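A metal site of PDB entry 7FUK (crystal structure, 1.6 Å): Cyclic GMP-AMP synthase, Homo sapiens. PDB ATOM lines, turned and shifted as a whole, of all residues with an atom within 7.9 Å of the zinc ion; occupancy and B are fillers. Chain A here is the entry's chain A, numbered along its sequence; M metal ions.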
ATOM      1  N   LEU A 227      25.199  28.232 -31.072  1.00  0.00           N
ATOM      2  CA  LEU A 227      24.919  29.398 -30.222  1.00  0.00           C
ATOM      3  C   LEU A 227      23.423  29.520 -29.919  1.00  0.00           C
ATOM      4  O   LEU A 227      23.036  29.874 -28.805  1.00  0.00           O
ATOM      5  CB  LEU A 227      25.449  30.670 -30.885  1.00  0.00           C
ATOM      6  CG  LEU A 227      25.342  31.947 -30.029  1.00  0.00           C
ATOM      7  CD1 LEU A 227      25.976  31.740 -28.693  1.00  0.00           C
ATOM      8  CD2 LEU A 227      25.985  33.122 -30.748  1.00  0.00           C
ATOM      9  N   ASN A 229      21.358  26.883 -29.968  1.00  0.00           N
ATOM     10  CA  ASN A 229      20.874  25.594 -29.501  1.00  0.00           C
ATOM     11  C   ASN A 229      21.944  25.119 -28.527  1.00  0.00           C
ATOM     12  O   ASN A 229      22.638  24.144 -28.736  1.00  0.00           O
ATOM     13  CB  ASN A 229      20.639  24.641 -30.675  1.00  0.00           C
ATOM     14  CG  ASN A 229      19.841  23.417 -30.255  1.00  0.00           C
ATOM     15  OD1 ASN A 229      19.615  23.172 -29.071  1.00  0.00           O
ATOM     16  ND2 ASN A 229      19.397  22.647 -31.225  1.00  0.00           N
ATOM     17  N   HIS A 230      22.106  25.890 -27.448  1.00  0.00           N
ATOM     18  CA  HIS A 230      23.341  25.936 -26.676  1.00  0.00           C
ATOM     19  C   HIS A 230      23.295  25.195 -25.337  1.00  0.00           C
ATOM     20  O   HIS A 230      24.278  25.245 -24.613  1.00  0.00           O
ATOM     21  CB  HIS A 230      23.716  27.396 -26.388  1.00  0.00           C
ATOM     22  CG  HIS A 230      22.633  28.140 -25.662  1.00  0.00           C
ATOM     23  ND1 HIS A 230      22.005  29.243 -26.200  1.00  0.00           N
ATOM     24  CD2 HIS A 230      22.045  27.927 -24.456  1.00  0.00           C
ATOM     25  CE1 HIS A 230      21.091  29.679 -25.351  1.00  0.00           C
ATOM     26  NE2 HIS A 230      21.073  28.881 -24.297  1.00  0.00           N
ATOM     27  N   GLY A 231      22.150  24.621 -24.944  1.00  0.00           N
ATOM     28  CA  GLY A 231      22.020  24.069 -23.613  1.00  0.00           C
ATOM     29  C   GLY A 231      22.252  22.574 -23.592  1.00  0.00           C
ATOM     30  O   GLY A 231      22.148  21.919 -24.624  1.00  0.00           O
ATOM     31  N   LYS A 232      22.587  22.039 -22.418  1.00  0.00           N
ATOM     32  CA  LYS A 232      22.446  20.592 -22.257  1.00  0.00           C
ATOM     33  C   LYS A 232      20.990  20.197 -22.431  1.00  0.00           C
ATOM     34  O   LYS A 232      20.681  19.188 -23.094  1.00  0.00           O
ATOM     35  CB  LYS A 232      22.957  20.142 -20.895  1.00  0.00           C
ATOM     36  CG  LYS A 232      22.755  18.626 -20.704  1.00  0.00           C
ATOM     37  CD  LYS A 232      23.456  18.024 -19.499  1.00  0.00           C
ATOM     38  CE  LYS A 232      24.982  18.036 -19.697  1.00  0.00           C
ATOM     39  NZ  LYS A 232      25.457  17.369 -20.986  1.00  0.00           N
ATOM     40  N   SER A 233      20.076  20.959 -21.854  1.00  0.00           N
ATOM     41  CA  SER A 233      18.654  20.739 -22.077  1.00  0.00           C
ATOM     42  C   SER A 233      18.289  21.232 -23.472  1.00  0.00           C
ATOM     43  O   SER A 233      18.658  22.343 -23.876  1.00  0.00           O
ATOM     44  CB  SER A 233      17.819  21.459 -21.019  1.00  0.00           C
ATOM     45  OG  SER A 233      16.443  21.438 -21.402  1.00  0.00           O
ATOM     46  N   THR A 235      15.501  22.271 -24.257  1.00  0.00           N
ATOM     47  CA  THR A 235      14.662  23.452 -24.103  1.00  0.00           C
ATOM     48  C   THR A 235      15.329  24.573 -23.300  1.00  0.00           C
ATOM     49  O   THR A 235      14.621  25.466 -22.796  1.00  0.00           O
ATOM     50  CB  THR A 235      13.313  23.085 -23.467  1.00  0.00           C
ATOM     51  OG1 THR A 235      13.503  22.280 -22.297  1.00  0.00           O
ATOM     52  CG2 THR A 235      12.425  22.299 -24.449  1.00  0.00           C
ATOM     53  N   CYS A 236      16.673  24.596 -23.221  1.00  0.00           N
ATOM     54  CA  CYS A 236      17.359  25.745 -22.629  1.00  0.00           C
ATOM     55  C   CYS A 236      16.943  27.034 -23.344  1.00  0.00           C
ATOM     56  O   CYS A 236      16.910  27.088 -24.576  1.00  0.00           O
ATOM     57  CB  CYS A 236      18.880  25.581 -22.736  1.00  0.00           C
ATOM     58  SG  CYS A 236      19.830  26.738 -21.693  1.00  0.00           S
ATOM     59  N   CYS A 237      16.552  28.044 -22.553  1.00  0.00           N
ATOM     60  CA  CYS A 237      16.110  29.345 -23.049  1.00  0.00           C
ATOM     61  C   CYS A 237      14.863  29.297 -23.953  1.00  0.00           C
ATOM     62  O   CYS A 237      14.537  30.290 -24.612  1.00  0.00           O
ATOM     63  CB  CYS A 237      17.288  30.065 -23.740  1.00  0.00           C
ATOM     64  SG  CYS A 237      18.580  30.629 -22.574  1.00  0.00           S
ATOM     65  N   GLU A 238      14.114  28.189 -23.979  1.00  0.00           N
ATOM     66  CA  GLU A 238      12.818  28.109 -24.664  1.00  0.00           C
ATOM     67  C   GLU A 238      11.636  28.302 -23.729  1.00  0.00           C
ATOM     68  O   GLU A 238      10.489  28.284 -24.196  1.00  0.00           O
ATOM     69  CB  GLU A 238      12.644  26.770 -25.417  1.00  0.00           C
ATOM     70  CG  GLU A 238      13.413  26.691 -26.731  1.00  0.00           C
ATOM     71  CD  GLU A 238      12.930  25.560 -27.680  1.00  0.00           C
ATOM     72  OE1 GLU A 238      12.031  24.761 -27.315  1.00  0.00           O
ATOM     73  OE2 GLU A 238      13.462  25.485 -28.791  1.00  0.00           O
ATOM     74  N   GLU A 242      13.979  27.925 -17.753  1.00  0.00           N
ATOM     75  CA  GLU A 242      15.302  27.499 -18.181  1.00  0.00           C
ATOM     76  C   GLU A 242      16.007  28.656 -18.884  1.00  0.00           C
ATOM     77  O   GLU A 242      16.198  28.647 -20.095  1.00  0.00           O
ATOM     78  CB  GLU A 242      15.219  26.276 -19.095  1.00  0.00           C
ATOM     79  CG  GLU A 242      14.520  25.071 -18.518  1.00  0.00           C
ATOM     80  CD  GLU A 242      14.583  23.909 -19.486  1.00  0.00           C
ATOM     81  OE1 GLU A 242      15.725  23.500 -19.827  1.00  0.00           O
ATOM     82  OE2 GLU A 242      13.519  23.477 -19.960  1.00  0.00           O
ATOM     83  N   LYS A 243      16.411  29.659 -18.103  1.00  0.00           N
ATOM     84  CA  LYS A 243      17.081  30.842 -18.640  1.00  0.00           C
ATOM     85  C   LYS A 243      18.543  30.777 -18.245  1.00  0.00           C
ATOM     86  O   LYS A 243      18.871  30.792 -17.046  1.00  0.00           O
ATOM     87  CB  LYS A 243      16.426  32.113 -18.105  1.00  0.00           C
ATOM     88  CG  LYS A 243      15.033  32.362 -18.647  1.00  0.00           C
ATOM     89  CD  LYS A 243      15.077  32.654 -20.139  1.00  0.00           C
ATOM     90  CE  LYS A 243      13.705  32.472 -20.783  1.00  0.00           C
ATOM     91  NZ  LYS A 243      13.750  32.580 -22.273  1.00  0.00           N
ATOM     92  N   CYS A 244      19.437  30.674 -19.217  1.00  0.00           N
ATOM     93  CA  CYS A 244      20.854  30.665 -18.910  1.00  0.00           C
ATOM     94  C   CYS A 244      21.489  31.968 -19.396  1.00  0.00           C
ATOM     95  O   CYS A 244      20.878  32.755 -20.124  1.00  0.00           O
ATOM     96  CB  CYS A 244      21.566  29.448 -19.534  1.00  0.00           C
ATOM     97  SG  CYS A 244      21.966  29.598 -21.282  1.00  0.00           S
ATOM     98  N   CYS A 245      22.752  32.173 -19.024  1.00  0.00           N
ATOM     99  CA  CYS A 245      23.437  33.399 -19.431  1.00  0.00           C
ATOM    100  C   CYS A 245      24.542  33.154 -20.459  1.00  0.00           C
ATOM    101  O   CYS A 245      25.398  34.011 -20.620  1.00  0.00           O
ATOM    102  CB  CYS A 245      24.013  34.129 -18.209  1.00  0.00           C
ATOM    103  SG  CYS A 245      25.248  33.244 -17.247  1.00  0.00           S
ATOM    104  N   ARG A 246      24.512  32.026 -21.184  1.00  0.00           N
ATOM    105  CA  ARG A 246      25.587  31.761 -22.152  1.00  0.00           C
ATOM    106  C   ARG A 246      25.712  32.873 -23.197  1.00  0.00           C
ATOM    107  O   ARG A 246      26.808  33.431 -23.422  1.00  0.00           O
ATOM    108  CB  ARG A 246      25.359  30.410 -22.818  1.00  0.00           C
ATOM    109  CG  ARG A 246      25.602  29.210 -21.880  1.00  0.00           C
ATOM    110  CD  ARG A 246      25.532  27.945 -22.710  1.00  0.00           C
ATOM    111  NE  ARG A 246      25.758  26.695 -21.992  1.00  0.00           N
ATOM    112  CZ  ARG A 246      24.807  26.022 -21.327  1.00  0.00           C
ATOM    113  NH1 ARG A 246      25.090  24.843 -20.750  1.00  0.00           N
ATOM    114  NH2 ARG A 246      23.571  26.539 -21.241  1.00  0.00           N
ATOM    115  N   LYS A 247      24.613  33.225 -23.854  1.00  0.00           N
ATOM    116  CA  LYS A 247      24.677  34.224 -24.917  1.00  0.00           C
ATOM    117  C   LYS A 247      25.127  35.573 -24.375  1.00  0.00           C
ATOM    118  O   LYS A 247      25.885  36.304 -25.038  1.00  0.00           O
ATOM    119  CB  LYS A 247      23.328  34.389 -25.601  1.00  0.00           C
ATOM    120  CG  LYS A 247      23.022  33.322 -26.631  1.00  0.00           C
ATOM    121  CD  LYS A 247      21.708  33.652 -27.353  1.00  0.00           C
ATOM    122  CE  LYS A 247      21.504  32.754 -28.548  1.00  0.00           C
ATOM    123  NZ  LYS A 247      20.117  32.861 -29.100  1.00  0.00           N
ATOM    124  N   ASP A 292      23.736  23.226 -17.534  1.00  0.00           N
ATOM    125  CA  ASP A 292      22.990  24.486 -17.608  1.00  0.00           C
ATOM    126  C   ASP A 292      22.992  25.199 -16.257  1.00  0.00           C
ATOM    127  O   ASP A 292      22.984  26.442 -16.215  1.00  0.00           O
ATOM    128  CB  ASP A 292      21.559  24.226 -18.071  1.00  0.00           C
ATOM    129  CG  ASP A 292      21.501  23.682 -19.488  1.00  0.00           C
ATOM    130  OD1 ASP A 292      22.477  23.895 -20.232  1.00  0.00           O
ATOM    131  OD2 ASP A 292      20.488  23.042 -19.865  1.00  0.00           O
ATOM    132  N   TRP A 295      25.400  27.919 -15.755  1.00  0.00           N
ATOM    133  CA  TRP A 295      25.172  29.180 -16.465  1.00  0.00           C
ATOM    134  C   TRP A 295      23.864  29.811 -16.039  1.00  0.00           C
ATOM    135  O   TRP A 295      23.162  30.445 -16.835  1.00  0.00           O
ATOM    136  CB  TRP A 295      25.186  28.956 -17.977  1.00  0.00           C
ATOM    137  CG  TRP A 295      26.467  28.394 -18.489  1.00  0.00           C
ATOM    138  CD1 TRP A 295      26.837  27.069 -18.549  1.00  0.00           C
ATOM    139  CD2 TRP A 295      27.574  29.157 -18.977  1.00  0.00           C
ATOM    140  NE1 TRP A 295      28.128  26.968 -19.049  1.00  0.00           N
ATOM    141  CE2 TRP A 295      28.583  28.236 -19.326  1.00  0.00           C
ATOM    142  CE3 TRP A 295      27.810  30.530 -19.126  1.00  0.00           C
ATOM    143  CZ2 TRP A 295      29.816  28.650 -19.873  1.00  0.00           C
ATOM    144  CZ3 TRP A 295      29.042  30.953 -19.683  1.00  0.00           C
ATOM    145  CH2 TRP A 295      30.034  30.009 -20.022  1.00  0.00           C
HETATM  146 ZN    ZN M   1      20.112  28.849 -22.538  1.00  0.00          ZN
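Within 4 Å of the zinc ion: His 230, Cys 236, Cys 237 and Cys 244.
The nearest printed residue that does not touch the zinc ion is Arg 246 (4.4 Å).
O of His 230 is in hydrogen-bond range of NE of Arg 246, at 3.3 Å.
The backbone carbonyl oxygen (O) of Cys 237 is in hydrogen-bond range of the side-chain amino group (NZ) of Lys 243.
The side-chain sulfur (SG) of Cys 236 sits close to the guanidinium group (NH2) of Arg 246 (3.8 Å).
ND1 of His 230 is in hydrogen-bond range of O of Leu 227, at 2.9 Å.
The backbone carbonyl oxygen (O) of Glu 242 lies within hydrogen-bond range of the backbone NH (N) of Cys 237 (2.6 Å).
NH2 of Arg 246 sits close to SG of Cys 244, 3.5 Å away.
The zinc ion is bound by a ring nitrogen (NE2) of His 230 (2.0 Å), the side-chain sulfur of Cys 236 (2.3 Å), the side-chain sulfur of Cys 237 (2.3 Å) and the side-chain sulfur of Cys 244 (2.4 Å).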
